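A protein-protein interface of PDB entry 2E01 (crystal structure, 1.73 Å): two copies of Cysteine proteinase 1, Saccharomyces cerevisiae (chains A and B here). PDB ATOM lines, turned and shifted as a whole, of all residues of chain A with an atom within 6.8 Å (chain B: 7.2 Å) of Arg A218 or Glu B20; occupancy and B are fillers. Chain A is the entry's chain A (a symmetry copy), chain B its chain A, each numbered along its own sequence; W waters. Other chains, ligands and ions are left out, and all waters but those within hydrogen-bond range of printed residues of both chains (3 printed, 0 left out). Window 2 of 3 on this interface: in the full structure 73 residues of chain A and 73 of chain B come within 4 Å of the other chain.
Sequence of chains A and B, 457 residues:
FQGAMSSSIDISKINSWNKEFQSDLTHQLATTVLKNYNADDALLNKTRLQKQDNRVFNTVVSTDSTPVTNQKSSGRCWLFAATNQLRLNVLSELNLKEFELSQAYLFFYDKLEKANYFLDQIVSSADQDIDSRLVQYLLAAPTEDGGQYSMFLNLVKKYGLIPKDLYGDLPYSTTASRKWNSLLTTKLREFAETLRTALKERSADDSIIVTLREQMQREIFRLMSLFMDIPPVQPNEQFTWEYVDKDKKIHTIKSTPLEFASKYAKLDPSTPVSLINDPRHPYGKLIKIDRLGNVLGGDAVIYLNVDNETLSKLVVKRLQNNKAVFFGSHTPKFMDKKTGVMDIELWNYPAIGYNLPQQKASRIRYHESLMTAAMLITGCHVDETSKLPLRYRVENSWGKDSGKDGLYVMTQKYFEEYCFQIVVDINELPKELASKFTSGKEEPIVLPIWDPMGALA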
ATOM      1  N   ARG A 213      19.039 -10.293 -22.098  1.00  0.00           N
ATOM      2  CA  ARG A 213      17.862 -10.560 -21.288  1.00  0.00           C
ATOM      3  C   ARG A 213      16.890 -11.463 -22.017  1.00  0.00           C
ATOM      4  O   ARG A 213      16.306 -12.340 -21.415  1.00  0.00           O
ATOM      5  CB  ARG A 213      17.144  -9.269 -20.872  1.00  0.00           C
ATOM      6  CG  ARG A 213      17.982  -8.436 -19.851  1.00  0.00           C
ATOM      7  CD  ARG A 213      17.287  -7.173 -19.467  1.00  0.00           C
ATOM      8  NE  ARG A 213      16.124  -7.398 -18.621  1.00  0.00           N
ATOM      9  CZ  ARG A 213      15.543  -6.452 -17.898  1.00  0.00           C
ATOM     10  NH1 ARG A 213      16.030  -5.209 -17.918  1.00  0.00           N
ATOM     11  NH2 ARG A 213      14.460  -6.737 -17.178  1.00  0.00           N
ATOM     12  N   GLU A 214      16.743 -11.273 -23.328  1.00  0.00           N
ATOM     13  CA  GLU A 214      15.796 -12.130 -24.040  1.00  0.00           C
ATOM     14  C   GLU A 214      16.319 -13.557 -24.123  1.00  0.00           C
ATOM     15  O   GLU A 214      15.541 -14.506 -24.051  1.00  0.00           O
ATOM     16  CB  GLU A 214      15.526 -11.607 -25.444  1.00  0.00           C
ATOM     17  CG  GLU A 214      14.336 -12.318 -26.053  1.00  0.00           C
ATOM     18  CD  GLU A 214      13.973 -11.797 -27.427  1.00  0.00           C
ATOM     19  OE1 GLU A 214      14.855 -11.799 -28.322  1.00  0.00           O
ATOM     20  OE2 GLU A 214      12.817 -11.390 -27.595  1.00  0.00           O
ATOM     21  N   GLN A 215      17.621 -13.706 -24.286  1.00  0.00           N
ATOM     22  CA  GLN A 215      18.214 -15.039 -24.335  1.00  0.00           C
ATOM     23  C   GLN A 215      18.030 -15.749 -22.970  1.00  0.00           C
ATOM     24  O   GLN A 215      17.871 -16.963 -22.911  1.00  0.00           O
ATOM     25  CB  GLN A 215      19.700 -14.932 -24.661  1.00  0.00           C
ATOM     26  CG  GLN A 215      19.960 -14.593 -26.111  1.00  0.00           C
ATOM     27  CD  GLN A 215      21.422 -14.193 -26.348  1.00  0.00           C
ATOM     28  OE1 GLN A 215      22.200 -13.968 -25.396  1.00  0.00           O
ATOM     29  NE2 GLN A 215      21.798 -14.088 -27.619  1.00  0.00           N
ATOM     30  N   MET A 216      18.072 -14.974 -21.893  1.00  0.00           N
ATOM     31  CA  MET A 216      17.896 -15.543 -20.552  1.00  0.00           C
ATOM     32  C   MET A 216      16.453 -15.983 -20.366  1.00  0.00           C
ATOM     33  O   MET A 216      16.194 -17.050 -19.832  1.00  0.00           O
ATOM     34  CB  MET A 216      18.318 -14.499 -19.489  1.00  0.00           C
ATOM     35  CG  MET A 216      19.818 -14.309 -19.503  1.00  0.00           C
ATOM     36  SD  MET A 216      20.308 -12.923 -18.427  1.00  0.00           S
ATOM     37  CE  MET A 216      21.987 -13.150 -18.602  1.00  0.00           C
ATOM     38  N   GLN A 217      15.503 -15.189 -20.876  1.00  0.00           N
ATOM     39  CA  GLN A 217      14.102 -15.551 -20.755  1.00  0.00           C
ATOM     40  C   GLN A 217      13.913 -16.869 -21.504  1.00  0.00           C
ATOM     41  O   GLN A 217      13.188 -17.770 -21.056  1.00  0.00           O
ATOM     42  CB  GLN A 217      13.176 -14.519 -21.420  1.00  0.00           C
ATOM     43  CG  GLN A 217      12.994 -13.204 -20.738  1.00  0.00           C
ATOM     44  CD  GLN A 217      11.855 -12.409 -21.387  1.00  0.00           C
ATOM     45  OE1 GLN A 217      11.524 -12.634 -22.568  1.00  0.00           O
ATOM     46  NE2 GLN A 217      11.257 -11.491 -20.634  1.00  0.00           N
ATOM     47  N   ARG A 218      14.546 -16.953 -22.672  1.00  0.00           N
ATOM     48  CA  ARG A 218      14.419 -18.153 -23.493  1.00  0.00           C
ATOM     49  C   ARG A 218      14.976 -19.390 -22.775  1.00  0.00           C
ATOM     50  O   ARG A 218      14.361 -20.456 -22.807  1.00  0.00           O
ATOM     51  CB  ARG A 218      15.139 -17.925 -24.818  1.00  0.00           C
ATOM     52  CG  ARG A 218      14.930 -18.997 -25.868  1.00  0.00           C
ATOM     53  CD  ARG A 218      15.588 -18.529 -27.165  1.00  0.00           C
ATOM     54  NE  ARG A 218      15.433 -19.473 -28.277  1.00  0.00           N
ATOM     55  CZ  ARG A 218      16.237 -20.512 -28.422  1.00  0.00           C
ATOM     56  NH1 ARG A 218      17.201 -20.697 -27.526  1.00  0.00           N
ATOM     57  NH2 ARG A 218      16.114 -21.344 -29.449  1.00  0.00           N
ATOM     58  N   GLU A 219      16.147 -19.242 -22.147  1.00  0.00           N
ATOM     59  CA  GLU A 219      16.757 -20.359 -21.423  1.00  0.00           C
ATOM     60  C   GLU A 219      15.919 -20.731 -20.207  1.00  0.00           C
ATOM     61  O   GLU A 219      15.741 -21.916 -19.906  1.00  0.00           O
ATOM     62  CB  GLU A 219      18.199 -20.026 -20.999  1.00  0.00           C
ATOM     63  CG  GLU A 219      18.977 -21.272 -20.660  1.00  0.00           C
ATOM     64  CD  GLU A 219      19.341 -22.113 -21.892  1.00  0.00           C
ATOM     65  OE1 GLU A 219      18.708 -21.982 -22.987  1.00  0.00           O
ATOM     66  OE2 GLU A 219      20.277 -22.916 -21.743  1.00  0.00           O
ATOM     67  N   ILE A 220      15.358 -19.733 -19.530  1.00  0.00           N
ATOM     68  CA  ILE A 220      14.494 -20.036 -18.377  1.00  0.00           C
ATOM     69  C   ILE A 220      13.282 -20.863 -18.862  1.00  0.00           C
ATOM     70  O   ILE A 220      12.908 -21.862 -18.270  1.00  0.00           O
ATOM     71  CB  ILE A 220      14.004 -18.716 -17.711  1.00  0.00           C
ATOM     72  CG1 ILE A 220      15.175 -18.028 -16.988  1.00  0.00           C
ATOM     73  CG2 ILE A 220      12.853 -18.977 -16.765  1.00  0.00           C
ATOM     74  CD1 ILE A 220      14.789 -16.572 -16.608  1.00  0.00           C
ATOM     75  N   PHE A 221      12.639 -20.404 -19.943  1.00  0.00           N
ATOM     76  CA  PHE A 221      11.478 -21.102 -20.473  1.00  0.00           C
ATOM     77  C   PHE A 221      11.842 -22.508 -20.932  1.00  0.00           C
ATOM     78  O   PHE A 221      11.082 -23.442 -20.684  1.00  0.00           O
ATOM     79  CB  PHE A 221      10.862 -20.348 -21.685  1.00  0.00           C
ATOM     80  CG  PHE A 221       9.638 -21.047 -22.242  1.00  0.00           C
ATOM     81  CD1 PHE A 221       8.475 -21.103 -21.480  1.00  0.00           C
ATOM     82  CD2 PHE A 221       9.738 -21.832 -23.394  1.00  0.00           C
ATOM     83  CE1 PHE A 221       7.407 -21.953 -21.845  1.00  0.00           C
ATOM     84  CE2 PHE A 221       8.665 -22.697 -23.762  1.00  0.00           C
ATOM     85  CZ  PHE A 221       7.528 -22.742 -22.986  1.00  0.00           C
ATOM     86  N   ARG A 222      12.988 -22.654 -21.587  1.00  0.00           N
ATOM     87  CA  ARG A 222      13.409 -23.964 -22.062  1.00  0.00           C
ATOM     88  C   ARG A 222      13.534 -24.919 -20.861  1.00  0.00           C
ATOM     89  O   ARG A 222      13.012 -26.048 -20.867  1.00  0.00           O
ATOM     90  CB  ARG A 222      14.769 -23.907 -22.789  1.00  0.00           C
ATOM     91  CG  ARG A 222      15.125 -25.265 -23.449  1.00  0.00           C
ATOM     92  CD  ARG A 222      16.432 -25.147 -24.223  1.00  0.00           C
ATOM     93  NE  ARG A 222      17.552 -24.867 -23.333  1.00  0.00           N
ATOM     94  CZ  ARG A 222      18.230 -25.792 -22.653  1.00  0.00           C
ATOM     95  NH1 ARG A 222      17.914 -27.086 -22.750  1.00  0.00           N
ATOM     96  NH2 ARG A 222      19.240 -25.414 -21.868  1.00  0.00           N
ATOM     97  N   LEU A 223      14.231 -24.456 -19.839  1.00  0.00           N
ATOM     98  CA  LEU A 223      14.421 -25.281 -18.665  1.00  0.00           C
ATOM     99  C   LEU A 223      13.087 -25.606 -18.001  1.00  0.00           C
ATOM    100  O   LEU A 223      12.851 -26.772 -17.661  1.00  0.00           O
ATOM    101  CB  LEU A 223      15.412 -24.617 -17.691  1.00  0.00           C
ATOM    102  CG  LEU A 223      16.834 -24.703 -18.309  1.00  0.00           C
ATOM    103  CD1 LEU A 223      17.768 -23.916 -17.432  1.00  0.00           C
ATOM    104  CD2 LEU A 223      17.365 -26.131 -18.475  1.00  0.00           C
ATOM    105  N   ILE B   9       7.280 -11.096 -19.951  1.00  0.00           N
ATOM    106  CA  ILE B   9       7.092 -12.409 -20.518  1.00  0.00           C
ATOM    107  C   ILE B   9       5.997 -12.206 -21.609  1.00  0.00           C
ATOM    108  O   ILE B   9       4.860 -11.780 -21.315  1.00  0.00           O
ATOM    109  CB  ILE B   9       6.542 -13.421 -19.448  1.00  0.00           C
ATOM    110  CG1 ILE B   9       7.710 -13.844 -18.519  1.00  0.00           C
ATOM    111  CG2 ILE B   9       5.868 -14.615 -20.151  1.00  0.00           C
ATOM    112  CD1 ILE B   9       8.833 -14.558 -19.295  1.00  0.00           C
ATOM    113  N   LYS B  13       5.927 -15.152 -27.616  1.00  0.00           N
ATOM    114  CA  LYS B  13       7.323 -15.583 -27.591  1.00  0.00           C
ATOM    115  C   LYS B  13       7.483 -16.968 -26.971  1.00  0.00           C
ATOM    116  O   LYS B  13       8.132 -17.828 -27.536  1.00  0.00           O
ATOM    117  CB  LYS B  13       8.163 -14.601 -26.752  1.00  0.00           C
ATOM    118  CG  LYS B  13       9.528 -14.320 -27.247  1.00  0.00           C
ATOM    119  CD  LYS B  13      10.102 -13.011 -26.632  1.00  0.00           C
ATOM    120  CE  LYS B  13       9.465 -11.777 -27.241  1.00  0.00           C
ATOM    121  NZ  LYS B  13      10.323 -10.544 -26.999  1.00  0.00           N
ATOM    122  N   ILE B  14       6.929 -17.152 -25.779  1.00  0.00           N
ATOM    123  CA  ILE B  14       7.120 -18.457 -25.138  1.00  0.00           C
ATOM    124  C   ILE B  14       6.447 -19.570 -25.893  1.00  0.00           C
ATOM    125  O   ILE B  14       6.972 -20.697 -25.928  1.00  0.00           O
ATOM    126  CB  ILE B  14       6.715 -18.460 -23.633  1.00  0.00           C
ATOM    127  CG1 ILE B  14       5.225 -18.154 -23.474  1.00  0.00           C
ATOM    128  CG2 ILE B  14       7.581 -17.424 -22.867  1.00  0.00           C
ATOM    129  CD1 ILE B  14       4.693 -18.220 -21.988  1.00  0.00           C
ATOM    130  N   ASN B  15       5.306 -19.301 -26.533  1.00  0.00           N
ATOM    131  CA  ASN B  15       4.700 -20.397 -27.278  1.00  0.00           C
ATOM    132  C   ASN B  15       5.470 -20.678 -28.588  1.00  0.00           C
ATOM    133  O   ASN B  15       5.501 -21.827 -29.070  1.00  0.00           O
ATOM    134  CB  ASN B  15       3.224 -20.080 -27.571  1.00  0.00           C
ATOM    135  CG  ASN B  15       2.326 -20.429 -26.408  1.00  0.00           C
ATOM    136  OD1 ASN B  15       1.837 -21.551 -26.322  1.00  0.00           O
ATOM    137  ND2 ASN B  15       2.099 -19.460 -25.502  1.00  0.00           N
ATOM    138  N   SER B  16       6.109 -19.651 -29.147  1.00  0.00           N
ATOM    139  CA  SER B  16       6.914 -19.845 -30.355  1.00  0.00           C
ATOM    140  C   SER B  16       8.185 -20.638 -29.987  1.00  0.00           C
ATOM    141  O   SER B  16       8.573 -21.590 -30.672  1.00  0.00           O
ATOM    142  CB  SER B  16       7.244 -18.488 -30.972  1.00  0.00           C
ATOM    143  OG  SER B  16       6.011 -17.854 -31.343  1.00  0.00           O
ATOM    144  N   TRP B  17       8.819 -20.257 -28.880  1.00  0.00           N
ATOM    145  CA  TRP B  17       9.992 -20.976 -28.409  1.00  0.00           C
ATOM    146  C   TRP B  17       9.616 -22.443 -28.141  1.00  0.00           C
ATOM    147  O   TRP B  17      10.344 -23.367 -28.487  1.00  0.00           O
ATOM    148  CB  TRP B  17      10.508 -20.335 -27.120  1.00  0.00           C
ATOM    149  CG  TRP B  17      11.151 -19.032 -27.347  1.00  0.00           C
ATOM    150  CD1 TRP B  17      11.710 -18.567 -28.526  1.00  0.00           C
ATOM    151  CD2 TRP B  17      11.312 -17.991 -26.381  1.00  0.00           C
ATOM    152  NE1 TRP B  17      12.204 -17.283 -28.338  1.00  0.00           N
ATOM    153  CE2 TRP B  17      11.973 -16.912 -27.029  1.00  0.00           C
ATOM    154  CE3 TRP B  17      10.958 -17.864 -25.021  1.00  0.00           C
ATOM    155  CZ2 TRP B  17      12.292 -15.721 -26.361  1.00  0.00           C
ATOM    156  CZ3 TRP B  17      11.281 -16.655 -24.341  1.00  0.00           C
ATOM    157  CH2 TRP B  17      11.939 -15.611 -25.019  1.00  0.00           C
ATOM    158  N   ASN B  18       8.482 -22.646 -27.499  1.00  0.00           N
ATOM    159  CA  ASN B  18       8.036 -24.001 -27.198  1.00  0.00           C
ATOM    160  C   ASN B  18       7.926 -24.822 -28.489  1.00  0.00           C
ATOM    161  O   ASN B  18       8.319 -25.976 -28.542  1.00  0.00           O
ATOM    162  CB  ASN B  18       6.691 -23.985 -26.496  1.00  0.00           C
ATOM    163  CG  ASN B  18       6.250 -25.376 -26.079  1.00  0.00           C
ATOM    164  OD1 ASN B  18       6.922 -26.006 -25.279  1.00  0.00           O
ATOM    165  ND2 ASN B  18       5.131 -25.869 -26.643  1.00  0.00           N
ATOM    166  N   LYS B  19       7.361 -24.228 -29.545  1.00  0.00           N
ATOM    167  CA  LYS B  19       7.275 -24.969 -30.803  1.00  0.00           C
ATOM    168  C   LYS B  19       8.663 -25.370 -31.321  1.00  0.00           C
ATOM    169  O   LYS B  19       8.875 -26.524 -31.809  1.00  0.00           O
ATOM    170  CB  LYS B  19       6.552 -24.126 -31.862  1.00  0.00           C
ATOM    171  CG  LYS B  19       6.470 -24.870 -33.191  1.00  0.00           C
ATOM    172  CD  LYS B  19       5.833 -23.985 -34.273  1.00  0.00           C
ATOM    173  CE  LYS B  19       5.675 -24.742 -35.613  1.00  0.00           C
ATOM    174  NZ  LYS B  19       5.286 -23.711 -36.631  1.00  0.00           N
ATOM    175  N   GLU B  20       9.615 -24.442 -31.248  1.00  0.00           N
ATOM    176  CA  GLU B  20      10.967 -24.729 -31.697  1.00  0.00           C
ATOM    177  C   GLU B  20      11.604 -25.853 -30.847  1.00  0.00           C
ATOM    178  O   GLU B  20      12.195 -26.797 -31.376  1.00  0.00           O
ATOM    179  CB  GLU B  20      11.814 -23.485 -31.571  1.00  0.00           C
ATOM    180  CG  GLU B  20      13.237 -23.709 -31.951  1.00  0.00           C
ATOM    181  CD  GLU B  20      14.073 -22.440 -31.868  1.00  0.00           C
ATOM    182  OE1 GLU B  20      13.512 -21.326 -32.024  1.00  0.00           O
ATOM    183  OE2 GLU B  20      15.301 -22.548 -31.662  1.00  0.00           O
ATOM    184  N   PHE B  21      11.462 -25.762 -29.536  1.00  0.00           N
ATOM    185  CA  PHE B  21      12.050 -26.811 -28.699  1.00  0.00           C
ATOM    186  C   PHE B  21      11.401 -28.166 -28.961  1.00  0.00           C
ATOM    187  O   PHE B  21      12.094 -29.182 -28.996  1.00  0.00           O
ATOM    188  CB  PHE B  21      11.922 -26.455 -27.211  1.00  0.00           C
ATOM    189  CG  PHE B  21      12.562 -25.159 -26.839  1.00  0.00           C
ATOM    190  CD1 PHE B  21      13.726 -24.720 -27.465  1.00  0.00           C
ATOM    191  CD2 PHE B  21      11.998 -24.365 -25.842  1.00  0.00           C
ATOM    192  CE1 PHE B  21      14.311 -23.497 -27.095  1.00  0.00           C
ATOM    193  CE2 PHE B  21      12.591 -23.161 -25.488  1.00  0.00           C
ATOM    194  CZ  PHE B  21      13.728 -22.732 -26.105  1.00  0.00           C
ATOM    195  N   GLN B  22      10.079 -28.201 -29.131  1.00  0.00           N
ATOM    196  CA  GLN B  22       9.385 -29.442 -29.399  1.00  0.00           C
ATOM    197  C   GLN B  22       9.809 -30.083 -30.728  1.00  0.00           C
ATOM    198  O   GLN B  22       9.590 -31.264 -30.933  1.00  0.00           O
ATOM    199  CB  GLN B  22       7.890 -29.229 -29.384  1.00  0.00           C
ATOM    200  CG  GLN B  22       7.307 -29.327 -28.009  1.00  0.00           C
ATOM    201  CD  GLN B  22       7.487 -30.736 -27.419  1.00  0.00           C
ATOM    202  OE1 GLN B  22       7.877 -30.883 -26.256  1.00  0.00           O
ATOM    203  NE2 GLN B  22       7.190 -31.776 -28.223  1.00  0.00           N
ATOM    204  N   SER B  23      10.465 -29.320 -31.598  1.00  0.00           N
ATOM    205  CA  SER B  23      10.923 -29.880 -32.871  1.00  0.00           C
ATOM    206  C   SER B  23      12.272 -30.598 -32.709  1.00  0.00           C
ATOM    207  O   SER B  23      12.747 -31.248 -33.627  1.00  0.00           O
ATOM    208  CB  SER B  23      11.053 -28.758 -33.939  1.00  0.00           C
ATOM    209  OG  SER B  23      12.243 -27.999 -33.770  1.00  0.00           O
ATOM    210  N   ASP B  24      12.893 -30.478 -31.539  1.00  0.00           N
ATOM    211  CA  ASP B  24      14.198 -31.096 -31.302  1.00  0.00           C
ATOM    212  C   ASP B  24      13.943 -32.434 -30.612  1.00  0.00           C
ATOM    213  O   ASP B  24      13.226 -32.505 -29.621  1.00  0.00           O
ATOM    214  CB  ASP B  24      15.058 -30.180 -30.431  1.00  0.00           C
ATOM    215  CG  ASP B  24      16.386 -30.802 -30.083  1.00  0.00           C
ATOM    216  OD1 ASP B  24      17.247 -30.942 -30.978  1.00  0.00           O
ATOM    217  OD2 ASP B  24      16.569 -31.172 -28.910  1.00  0.00           O
ATOM    218  N   LEU B  25      14.540 -33.492 -31.141  1.00  0.00           N
ATOM    219  CA  LEU B  25      14.316 -34.825 -30.618  1.00  0.00           C
ATOM    220  C   LEU B  25      14.824 -34.984 -29.179  1.00  0.00           C
ATOM    221  O   LEU B  25      14.232 -35.694 -28.376  1.00  0.00           O
ATOM    222  CB  LEU B  25      15.038 -35.835 -31.521  1.00  0.00           C
ATOM    223  CG  LEU B  25      14.548 -35.759 -32.972  1.00  0.00           C
ATOM    224  CD1 LEU B  25      15.546 -36.452 -33.937  1.00  0.00           C
ATOM    225  CD2 LEU B  25      13.133 -36.375 -33.029  1.00  0.00           C
ATOM    226  N   HIS B  27      15.034 -32.641 -26.875  1.00  0.00           N
ATOM    227  CA  HIS B  27      14.114 -31.940 -26.001  1.00  0.00           C
ATOM    228  C   HIS B  27      12.850 -32.761 -25.798  1.00  0.00           C
ATOM    229  O   HIS B  27      12.329 -32.825 -24.691  1.00  0.00           O
ATOM    230  CB  HIS B  27      13.709 -30.584 -26.609  1.00  0.00           C
ATOM    231  CG  HIS B  27      12.956 -29.711 -25.638  1.00  0.00           C
ATOM    232  ND1 HIS B  27      13.589 -28.860 -24.765  1.00  0.00           N
ATOM    233  CD2 HIS B  27      11.634 -29.551 -25.425  1.00  0.00           C
ATOM    234  CE1 HIS B  27      12.694 -28.202 -24.052  1.00  0.00           C
ATOM    235  NE2 HIS B  27      11.496 -28.600 -24.435  1.00  0.00           N
HETATM  236  O   HOH W   1      16.275 -28.688 -24.330  1.00  0.00           O
HETATM  237  O   HOH W   2      11.678 -10.525 -24.133  1.00  0.00           O
HETATM  238  O   HOH W   3      14.015 -14.966 -29.453  1.00  0.00           O
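The side-chain carboxylate of Glu A219 is in salt-bridge range of the guanidinium group of Arg A222, 2.7 Å away.
The backbone carbonyl oxygen (O) of Glu B20 lies within hydrogen-bond range of the side-chain hydroxyl (OG) of Ser B23 (2.7 Å).
The side-chain carboxylate (OD2) of Asp B24 is in hydrogen-bond range of the backbone NH (N) of His B27, at 2.9 Å.
No position is printed for both chains.
Of the 11 pairs that touch across the chains among the printed residues, none has its exchanged pair printed and touching as well.
Water W2 bridges OE1 of Gln A217 (2.6 Å) and NZ of Lys B13 (3.2 Å).
Water W1 lies within hydrogen-bond range of a ring nitrogen (ND1) of His B27 and the guanidinium group of Arg A222.
Water W3 bridges the indole nitrogen (NE1) of Trp B17 (3.1 Å) and the side-chain carboxylate (OE1) of Glu A214 (3.5 Å).
The side-chain amino group of Lys B13 lies within salt-bridge range of the side-chain carboxylate of Glu A214 (2.7 Å).
The side-chain carboxylate of Glu B20 lies within salt-bridge range of the guanidinium group of Arg A218 (2.6 Å).
Of the 15 printed residues of chain B, 7 touch a printed residue of chain A.
Hydrophobic or aromatic side chains of chain B that line the printed part of chain A: Ile B14, Trp B17, Phe B21 and His B27.
Along chain B the printed residues that touch a printed residue of chain A span positions 13 to 27.
Among the printed residues, 11 pairs touch across the chains.
Glu B20 touches just one residue of chain A: Arg A218 (2.6 Å).
Of the printed residues of chain A, Lys B13 touches Glu A214 (2.7 Å).
Printed residues of chain A within 4 Å of Trp B17: Glu A214, Gln A217 and Arg A218.
Printed residues of chain B within 4 Å of Gln A217: Trp B17 (3.9 Å).
The nearest residue of chain B that does not touch Arg A218 is Ile B14 (6.9 Å).
The nearest printed residue of chain A that does not touch Trp B17 is Phe A221 (4.1 Å).
Among the printed residues, merely in contact across the chains: Glu A214 with Trp B17, Gln A217 with Trp B17, Arg A218 with Trp B17, Arg A218 with Phe B21, Phe A221 with Ile B14, Phe A221 with Asn B18, Phe A221 with Phe B21, Arg A222 with Phe B21 and Arg A222 with His B27.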
